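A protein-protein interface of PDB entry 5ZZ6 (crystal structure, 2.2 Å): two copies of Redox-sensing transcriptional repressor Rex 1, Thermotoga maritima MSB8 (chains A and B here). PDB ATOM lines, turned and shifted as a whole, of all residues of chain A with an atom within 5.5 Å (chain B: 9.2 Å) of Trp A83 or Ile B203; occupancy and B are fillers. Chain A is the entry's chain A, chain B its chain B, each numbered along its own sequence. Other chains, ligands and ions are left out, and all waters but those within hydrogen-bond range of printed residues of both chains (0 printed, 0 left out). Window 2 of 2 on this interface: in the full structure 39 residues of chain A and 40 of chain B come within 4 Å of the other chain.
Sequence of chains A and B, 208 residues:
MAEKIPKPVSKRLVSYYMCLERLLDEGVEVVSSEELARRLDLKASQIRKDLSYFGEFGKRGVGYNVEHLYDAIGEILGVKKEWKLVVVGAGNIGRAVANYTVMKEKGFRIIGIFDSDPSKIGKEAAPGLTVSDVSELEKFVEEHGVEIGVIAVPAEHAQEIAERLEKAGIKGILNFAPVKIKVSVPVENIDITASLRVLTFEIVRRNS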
ATOM      1  N   GLY A  78     -14.649 -27.897  24.488  1.00  0.00           N
ATOM      2  CA  GLY A  78     -13.913 -26.647  24.538  1.00  0.00           C
ATOM      3  C   GLY A  78     -13.955 -25.976  25.894  1.00  0.00           C
ATOM      4  O   GLY A  78     -14.197 -24.768  25.989  1.00  0.00           O
ATOM      5  N   LYS A  81     -11.725 -22.669  26.975  1.00  0.00           N
ATOM      6  CA  LYS A  81     -12.030 -21.308  26.557  1.00  0.00           C
ATOM      7  C   LYS A  81     -12.844 -20.584  27.621  1.00  0.00           C
ATOM      8  O   LYS A  81     -13.712 -21.172  28.273  1.00  0.00           O
ATOM      9  CB  LYS A  81     -12.789 -21.321  25.228  1.00  0.00           C
ATOM     10  CG  LYS A  81     -13.327 -19.961  24.798  1.00  0.00           C
ATOM     11  CD  LYS A  81     -13.782 -19.954  23.348  1.00  0.00           C
ATOM     12  CE  LYS A  81     -14.534 -18.674  23.013  1.00  0.00           C
ATOM     13  NZ  LYS A  81     -13.755 -17.455  23.353  1.00  0.00           N
ATOM     14  N   GLU A  82     -12.544 -19.303  27.810  1.00  0.00           N
ATOM     15  CA  GLU A  82     -13.351 -18.433  28.649  1.00  0.00           C
ATOM     16  C   GLU A  82     -14.344 -17.665  27.784  1.00  0.00           C
ATOM     17  O   GLU A  82     -14.086 -17.386  26.611  1.00  0.00           O
ATOM     18  CB  GLU A  82     -12.473 -17.461  29.437  1.00  0.00           C
ATOM     19  N   TRP A  83     -15.489 -17.329  28.375  1.00  0.00           N
ATOM     20  CA  TRP A  83     -16.582 -16.694  27.653  1.00  0.00           C
ATOM     21  C   TRP A  83     -17.023 -15.437  28.384  1.00  0.00           C
ATOM     22  O   TRP A  83     -17.215 -15.465  29.603  1.00  0.00           O
ATOM     23  CB  TRP A  83     -17.766 -17.656  27.502  1.00  0.00           C
ATOM     24  CG  TRP A  83     -17.471 -18.831  26.618  1.00  0.00           C
ATOM     25  CD1 TRP A  83     -16.899 -20.019  26.986  1.00  0.00           C
ATOM     26  CD2 TRP A  83     -17.730 -18.929  25.216  1.00  0.00           C
ATOM     27  NE1 TRP A  83     -16.795 -20.851  25.899  1.00  0.00           N
ATOM     28  CE2 TRP A  83     -17.293 -20.203  24.798  1.00  0.00           C
ATOM     29  CE3 TRP A  83     -18.297 -18.067  24.273  1.00  0.00           C
ATOM     30  CZ2 TRP A  83     -17.404 -20.633  23.478  1.00  0.00           C
ATOM     31  CZ3 TRP A  83     -18.403 -18.496  22.963  1.00  0.00           C
ATOM     32  CH2 TRP A  83     -17.959 -19.768  22.578  1.00  0.00           C
ATOM     33  N   LYS A  84     -17.180 -14.339  27.642  1.00  0.00           N
ATOM     34  CA  LYS A  84     -17.732 -13.117  28.212  1.00  0.00           C
ATOM     35  C   LYS A  84     -19.252 -13.186  28.175  1.00  0.00           C
ATOM     36  O   LYS A  84     -19.843 -13.526  27.144  1.00  0.00           O
ATOM     37  CB  LYS A  84     -17.247 -11.882  27.453  1.00  0.00           C
ATOM     38  CG  LYS A  84     -15.737 -11.752  27.312  1.00  0.00           C
ATOM     39  CD  LYS A  84     -15.354 -10.325  26.924  1.00  0.00           C
ATOM     40  CE  LYS A  84     -14.193 -10.292  25.938  1.00  0.00           C
ATOM     41  NZ  LYS A  84     -14.585 -10.790  24.584  1.00  0.00           N
ATOM     42  N   LEU A  85     -19.881 -12.862  29.302  1.00  0.00           N
ATOM     43  CA  LEU A  85     -21.326 -12.925  29.451  1.00  0.00           C
ATOM     44  C   LEU A  85     -21.875 -11.575  29.880  1.00  0.00           C
ATOM     45  O   LEU A  85     -21.207 -10.806  30.579  1.00  0.00           O
ATOM     46  CB  LEU A  85     -21.735 -13.979  30.489  1.00  0.00           C
ATOM     47  CG  LEU A  85     -21.911 -15.422  30.012  1.00  0.00           C
ATOM     48  CD1 LEU A  85     -20.606 -16.007  29.474  1.00  0.00           C
ATOM     49  CD2 LEU A  85     -22.454 -16.279  31.150  1.00  0.00           C
ATOM     50  N   GLY A 107     -15.092 -20.841  33.628  1.00  0.00           N
ATOM     51  CA  GLY A 107     -14.803 -20.230  32.349  1.00  0.00           C
ATOM     52  C   GLY A 107     -15.878 -19.324  31.790  1.00  0.00           C
ATOM     53  O   GLY A 107     -15.796 -18.954  30.613  1.00  0.00           O
ATOM     54  N   PHE A 108     -16.878 -18.953  32.586  1.00  0.00           N
ATOM     55  CA  PHE A 108     -17.959 -18.079  32.141  1.00  0.00           C
ATOM     56  C   PHE A 108     -17.935 -16.826  33.006  1.00  0.00           C
ATOM     57  O   PHE A 108     -18.318 -16.868  34.180  1.00  0.00           O
ATOM     58  CB  PHE A 108     -19.306 -18.800  32.218  1.00  0.00           C
ATOM     59  CG  PHE A 108     -19.315 -20.131  31.517  1.00  0.00           C
ATOM     60  CD1 PHE A 108     -19.497 -20.205  30.145  1.00  0.00           C
ATOM     61  CD2 PHE A 108     -19.126 -21.306  32.226  1.00  0.00           C
ATOM     62  CE1 PHE A 108     -19.497 -21.428  29.492  1.00  0.00           C
ATOM     63  CE2 PHE A 108     -19.125 -22.534  31.582  1.00  0.00           C
ATOM     64  CZ  PHE A 108     -19.315 -22.591  30.213  1.00  0.00           C
ATOM     65  N   ARG A 109     -17.481 -15.714  32.425  1.00  0.00           N
ATOM     66  CA  ARG A 109     -17.230 -14.477  33.158  1.00  0.00           C
ATOM     67  C   ARG A 109     -18.300 -13.454  32.803  1.00  0.00           C
ATOM     68  O   ARG A 109     -18.311 -12.917  31.688  1.00  0.00           O
ATOM     69  CB  ARG A 109     -15.834 -13.937  32.848  1.00  0.00           C
ATOM     70  N   ILE A 110     -19.186 -13.178  33.751  1.00  0.00           N
ATOM     71  CA  ILE A 110     -20.178 -12.121  33.588  1.00  0.00           C
ATOM     72  C   ILE A 110     -19.490 -10.782  33.816  1.00  0.00           C
ATOM     73  O   ILE A 110     -18.962 -10.521  34.902  1.00  0.00           O
ATOM     74  CB  ILE A 110     -21.354 -12.309  34.552  1.00  0.00           C
ATOM     75  CG1 ILE A 110     -21.992 -13.684  34.335  1.00  0.00           C
ATOM     76  CG2 ILE A 110     -22.371 -11.186  34.370  1.00  0.00           C
ATOM     77  CD1 ILE A 110     -22.926 -14.115  35.438  1.00  0.00           C
ATOM     78  N   GLU A 147     -19.959 -12.537  24.139  1.00  0.00           N
ATOM     79  CA  GLU A 147     -20.360 -13.667  23.307  1.00  0.00           C
ATOM     80  C   GLU A 147     -21.697 -14.268  23.716  1.00  0.00           C
ATOM     81  O   GLU A 147     -22.460 -14.711  22.849  1.00  0.00           O
ATOM     82  CB  GLU A 147     -19.279 -14.746  23.339  1.00  0.00           C
ATOM     83  CG  GLU A 147     -17.944 -14.283  22.785  1.00  0.00           C
ATOM     84  CD  GLU A 147     -16.764 -14.860  23.545  1.00  0.00           C
ATOM     85  OE1 GLU A 147     -16.759 -14.778  24.795  1.00  0.00           O
ATOM     86  OE2 GLU A 147     -15.843 -15.400  22.892  1.00  0.00           O
ATOM     87  N   ILE A 148     -22.015 -14.285  25.006  1.00  0.00           N
ATOM     88  CA  ILE A 148     -23.227 -14.926  25.496  1.00  0.00           C
ATOM     89  C   ILE A 148     -24.044 -13.907  26.273  1.00  0.00           C
ATOM     90  O   ILE A 148     -23.518 -13.225  27.158  1.00  0.00           O
ATOM     91  CB  ILE A 148     -22.903 -16.154  26.368  1.00  0.00           C
ATOM     92  CG1 ILE A 148     -22.230 -17.231  25.518  1.00  0.00           C
ATOM     93  CG2 ILE A 148     -24.167 -16.695  27.030  1.00  0.00           C
ATOM     94  CD1 ILE A 148     -21.630 -18.346  26.333  1.00  0.00           C
ATOM     95  N   LYS A 171     -23.051 -14.003  20.284  1.00  0.00           N
ATOM     96  CA  LYS A 171     -22.823 -15.329  19.712  1.00  0.00           C
ATOM     97  C   LYS A 171     -23.803 -16.380  20.221  1.00  0.00           C
ATOM     98  O   LYS A 171     -24.101 -17.338  19.500  1.00  0.00           O
ATOM     99  CB  LYS A 171     -21.391 -15.794  20.006  1.00  0.00           C
ATOM    100  N   GLY A 172     -24.304 -16.242  21.447  1.00  0.00           N
ATOM    101  CA  GLY A 172     -25.260 -17.205  21.959  1.00  0.00           C
ATOM    102  C   GLY A 172     -26.093 -16.604  23.066  1.00  0.00           C
ATOM    103  O   GLY A 172     -25.723 -15.594  23.668  1.00  0.00           O
ATOM    104  N   PRO A 186     -27.463 -19.622  18.407  1.00  0.00           N
ATOM    105  CA  PRO A 186     -27.934 -20.714  19.271  1.00  0.00           C
ATOM    106  C   PRO A 186     -28.509 -20.186  20.578  1.00  0.00           C
ATOM    107  O   PRO A 186     -27.979 -19.256  21.188  1.00  0.00           O
ATOM    108  CB  PRO A 186     -26.672 -21.550  19.513  1.00  0.00           C
ATOM    109  CG  PRO A 186     -25.789 -21.241  18.361  1.00  0.00           C
ATOM    110  CD  PRO A 186     -26.060 -19.807  17.998  1.00  0.00           C
ATOM    111  N   SER B 195     -25.887 -26.113  31.064  1.00  0.00           N
ATOM    112  CA  SER B 195     -26.592 -25.441  29.978  1.00  0.00           C
ATOM    113  C   SER B 195     -25.681 -24.451  29.261  1.00  0.00           C
ATOM    114  O   SER B 195     -25.776 -24.279  28.038  1.00  0.00           O
ATOM    115  CB  SER B 195     -27.840 -24.746  30.514  1.00  0.00           C
ATOM    116  OG  SER B 195     -28.880 -25.682  30.737  1.00  0.00           O
ATOM    117  N   LEU B 196     -24.790 -23.793  30.008  1.00  0.00           N
ATOM    118  CA  LEU B 196     -23.773 -22.966  29.378  1.00  0.00           C
ATOM    119  C   LEU B 196     -22.832 -23.802  28.521  1.00  0.00           C
ATOM    120  O   LEU B 196     -22.410 -23.359  27.443  1.00  0.00           O
ATOM    121  CB  LEU B 196     -22.995 -22.197  30.440  1.00  0.00           C
ATOM    122  CG  LEU B 196     -23.757 -20.973  30.938  1.00  0.00           C
ATOM    123  CD1 LEU B 196     -23.036 -20.314  32.103  1.00  0.00           C
ATOM    124  CD2 LEU B 196     -23.946 -19.989  29.791  1.00  0.00           C
ATOM    125  N   ARG B 197     -22.502 -25.014  28.971  1.00  0.00           N
ATOM    126  CA  ARG B 197     -21.592 -25.862  28.203  1.00  0.00           C
ATOM    127  C   ARG B 197     -22.259 -26.376  26.934  1.00  0.00           C
ATOM    128  O   ARG B 197     -21.612 -26.497  25.886  1.00  0.00           O
ATOM    129  CB  ARG B 197     -21.109 -27.033  29.058  1.00  0.00           C
ATOM    130  CG  ARG B 197     -20.343 -26.628  30.310  1.00  0.00           C
ATOM    131  CD  ARG B 197     -19.467 -27.765  30.802  1.00  0.00           C
ATOM    132  NE  ARG B 197     -18.790 -27.458  32.066  1.00  0.00           N
ATOM    133  CZ  ARG B 197     -17.686 -26.726  32.170  1.00  0.00           C
ATOM    134  NH1 ARG B 197     -17.128 -26.201  31.085  1.00  0.00           N
ATOM    135  NH2 ARG B 197     -17.141 -26.511  33.362  1.00  0.00           N
ATOM    136  N   VAL B 198     -23.546 -26.708  27.016  1.00  0.00           N
ATOM    137  CA  VAL B 198     -24.300 -27.045  25.817  1.00  0.00           C
ATOM    138  C   VAL B 198     -24.312 -25.864  24.856  1.00  0.00           C
ATOM    139  O   VAL B 198     -24.071 -26.021  23.652  1.00  0.00           O
ATOM    140  CB  VAL B 198     -25.722 -27.493  26.203  1.00  0.00           C
ATOM    141  CG1 VAL B 198     -26.574 -27.721  24.961  1.00  0.00           C
ATOM    142  CG2 VAL B 198     -25.653 -28.757  27.048  1.00  0.00           C
ATOM    143  N   LEU B 199     -24.550 -24.657  25.377  1.00  0.00           N
ATOM    144  CA  LEU B 199     -24.663 -23.484  24.518  1.00  0.00           C
ATOM    145  C   LEU B 199     -23.348 -23.186  23.807  1.00  0.00           C
ATOM    146  O   LEU B 199     -23.324 -22.945  22.594  1.00  0.00           O
ATOM    147  CB  LEU B 199     -25.113 -22.278  25.336  1.00  0.00           C
ATOM    148  CG  LEU B 199     -25.108 -20.955  24.579  1.00  0.00           C
ATOM    149  CD1 LEU B 199     -26.152 -20.945  23.471  1.00  0.00           C
ATOM    150  CD2 LEU B 199     -25.339 -19.817  25.558  1.00  0.00           C
ATOM    151  N   THR B 200     -22.240 -23.201  24.548  1.00  0.00           N
ATOM    152  CA  THR B 200     -20.945 -22.906  23.943  1.00  0.00           C
ATOM    153  C   THR B 200     -20.548 -23.974  22.935  1.00  0.00           C
ATOM    154  O   THR B 200     -19.919 -23.671  21.914  1.00  0.00           O
ATOM    155  CB  THR B 200     -19.882 -22.771  25.030  1.00  0.00           C
ATOM    156  OG1 THR B 200     -19.923 -23.925  25.880  1.00  0.00           O
ATOM    157  CG2 THR B 200     -20.153 -21.537  25.857  1.00  0.00           C
ATOM    158  N   PHE B 201     -20.901 -25.233  23.203  1.00  0.00           N
ATOM    159  CA  PHE B 201     -20.621 -26.274  22.223  1.00  0.00           C
ATOM    160  C   PHE B 201     -21.406 -26.042  20.936  1.00  0.00           C
ATOM    161  O   PHE B 201     -20.882 -26.267  19.839  1.00  0.00           O
ATOM    162  CB  PHE B 201     -20.931 -27.654  22.801  1.00  0.00           C
ATOM    163  CG  PHE B 201     -20.754 -28.769  21.809  1.00  0.00           C
ATOM    164  CD1 PHE B 201     -19.500 -29.301  21.559  1.00  0.00           C
ATOM    165  CD2 PHE B 201     -21.839 -29.268  21.108  1.00  0.00           C
ATOM    166  CE1 PHE B 201     -19.334 -30.321  20.641  1.00  0.00           C
ATOM    167  CE2 PHE B 201     -21.682 -30.285  20.190  1.00  0.00           C
ATOM    168  CZ  PHE B 201     -20.427 -30.813  19.957  1.00  0.00           C
ATOM    169  N   GLU B 202     -22.660 -25.594  21.045  1.00  0.00           N
ATOM    170  CA  GLU B 202     -23.424 -25.303  19.836  1.00  0.00           C
ATOM    171  C   GLU B 202     -22.903 -24.055  19.132  1.00  0.00           C
ATOM    172  O   GLU B 202     -22.962 -23.976  17.899  1.00  0.00           O
ATOM    173  CB  GLU B 202     -24.910 -25.162  20.167  1.00  0.00           C
ATOM    174  CG  GLU B 202     -25.571 -26.465  20.605  1.00  0.00           C
ATOM    175  CD  GLU B 202     -26.966 -26.260  21.183  1.00  0.00           C
ATOM    176  OE1 GLU B 202     -27.653 -27.274  21.450  1.00  0.00           O
ATOM    177  OE2 GLU B 202     -27.379 -25.092  21.375  1.00  0.00           O
ATOM    178  N   ILE B 203     -22.381 -23.085  19.893  1.00  0.00           N
ATOM    179  CA  ILE B 203     -21.758 -21.904  19.297  1.00  0.00           C
ATOM    180  C   ILE B 203     -20.550 -22.307  18.464  1.00  0.00           C
ATOM    181  O   ILE B 203     -20.408 -21.905  17.304  1.00  0.00           O
ATOM    182  CB  ILE B 203     -21.354 -20.894  20.386  1.00  0.00           C
ATOM    183  CG1 ILE B 203     -22.569 -20.174  20.971  1.00  0.00           C
ATOM    184  CG2 ILE B 203     -20.344 -19.896  19.837  1.00  0.00           C
ATOM    185  CD1 ILE B 203     -22.199 -19.179  22.074  1.00  0.00           C
ATOM    186  N   VAL B 204     -19.649 -23.092  19.056  1.00  0.00           N
ATOM    187  CA  VAL B 204     -18.473 -23.541  18.322  1.00  0.00           C
ATOM    188  C   VAL B 204     -18.874 -24.482  17.189  1.00  0.00           C
ATOM    189  O   VAL B 204     -18.226 -24.508  16.135  1.00  0.00           O
ATOM    190  CB  VAL B 204     -17.463 -24.193  19.288  1.00  0.00           C
ATOM    191  CG1 VAL B 204     -16.240 -24.702  18.533  1.00  0.00           C
ATOM    192  CG2 VAL B 204     -17.042 -23.201  20.364  1.00  0.00           C
ATOM    193  N   ARG B 205     -19.959 -25.243  17.366  1.00  0.00           N
ATOM    194  CA  ARG B 205     -20.377 -26.192  16.337  1.00  0.00           C
ATOM    195  C   ARG B 205     -20.737 -25.477  15.039  1.00  0.00           C
ATOM    196  O   ARG B 205     -20.449 -25.976  13.947  1.00  0.00           O
ATOM    197  CB  ARG B 205     -21.560 -27.023  16.840  1.00  0.00           C
ATOM    198  CG  ARG B 205     -21.721 -28.385  16.170  1.00  0.00           C
ATOM    199  CD  ARG B 205     -23.155 -28.892  16.286  1.00  0.00           C
ATOM    200  NE  ARG B 205     -24.099 -27.961  15.674  1.00  0.00           N
ATOM    201  CZ  ARG B 205     -24.301 -27.856  14.362  1.00  0.00           C
ATOM    202  NH1 ARG B 205     -23.624 -28.626  13.521  1.00  0.00           N
ATOM    203  NH2 ARG B 205     -25.176 -26.976  13.892  1.00  0.00           N
ATOM    204  N   ARG B 206     -21.354 -24.297  15.139  1.00  0.00           N
ATOM    205  CA  ARG B 206     -21.773 -23.554  13.957  1.00  0.00           C
ATOM    206  C   ARG B 206     -20.598 -23.068  13.113  1.00  0.00           C
ATOM    207  O   ARG B 206     -20.767 -22.861  11.907  1.00  0.00           O
ATOM    208  CB  ARG B 206     -22.648 -22.368  14.369  1.00  0.00           C
ATOM    209  N   ASN B 207     -19.418 -22.900  13.699  1.00  0.00           N
ATOM    210  CA  ASN B 207     -18.253 -22.458  12.936  1.00  0.00           C
ATOM    211  C   ASN B 207     -17.776 -23.530  11.963  1.00  0.00           C
ATOM    212  O   ASN B 207     -17.774 -23.321  10.749  1.00  0.00           O
ATOM    213  CB  ASN B 207     -17.112 -22.068  13.872  1.00  0.00           C
ATOM    214  CG  ASN B 207     -17.465 -20.890  14.751  1.00  0.00           C
ATOM    215  OD1 ASN B 207     -18.432 -20.171  14.486  1.00  0.00           O
ATOM    216  ND2 ASN B 207     -16.681 -20.681  15.805  1.00  0.00           N
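Of the 15 printed residues of chain A, 6 touch a printed residue of chain B. Hydrophobic or aromatic side chains of chain A that line the printed part of chain B: Trp A83, Phe A108, Ile A148 and Pro A186. Among the printed residues, no Asp or Glu carboxylate lies within 4 Å of a Lys or Arg side-chain nitrogen of the other chain.
N of Trp A83 lies within hydrogen-bond range of O of Gly A107, 2.8 Å away. The backbone NH of Arg A109 lies within hydrogen-bond range of the backbone carbonyl oxygen of Trp A83, at 2.8 Å. The backbone NH of Ile A148 is in hydrogen-bond range of the backbone carbonyl oxygen of Lys A84, at 3.1 Å. O of Glu A147 lies within hydrogen-bond range of N of Lys A171 (2.7 Å). The backbone carbonyl oxygen of Leu B196 sits at hydrogen-bond distance from the side-chain hydroxyl of Thr B200, 3.0 Å away. The backbone carbonyl oxygen of Arg B197 is in hydrogen-bond range of the side-chain hydroxyl of Thr B200.
No position is printed for both chains. Of the 11 pairs that touch across the chains among the printed residues, none has its exchanged pair printed and touching as well.
Among the printed residues, pairs that only touch across the chains: Trp A83 with Thr B200 (3.3 Å), Trp A83 with Ile B203 (3.6 Å), Phe A108 with Leu B196 (3.7 Å), Phe A108 with Thr B200 (3.7 Å), Ile A148 with Leu B199 (3.6 Å), Ile A148 with Thr B200 (3.5 Å), Ile A148 with Ile B203 (3.96 Å), Lys A171 with Ile B203 (3.5 Å), Gly A172 with Ile B203 (3.6 Å), Pro A186 with Leu B199 (3.4 Å) and Pro A186 with Glu B202 (3.96 Å).
No residue of chain B comes within 4 Å of Glu A82. Printed residues of chain B within 4 Å of Trp A83: Thr B200 (3.3 Å) and Ile B203 (3.6 Å). Arg A109 touches none of the printed residues of chain B. Of the printed residues of chain B, Ile A148 touches Leu B199 (3.6 Å), Thr B200 (3.5 Å) and Ile B203 (3.96 Å). Of the printed residues of chain B, Lys A171 touches Ile B203. Arg B197 touches none of the printed residues of chain A. Printed residues of chain A within 4 Å of Ile B203: Trp A83 (3.6 Å), Ile A148 (3.96 Å), Lys A171 (3.5 Å) and Gly A172 (3.6 Å). The nearest printed residue of chain B that does not touch Pro A186 is Ile B203 (4.2 Å).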
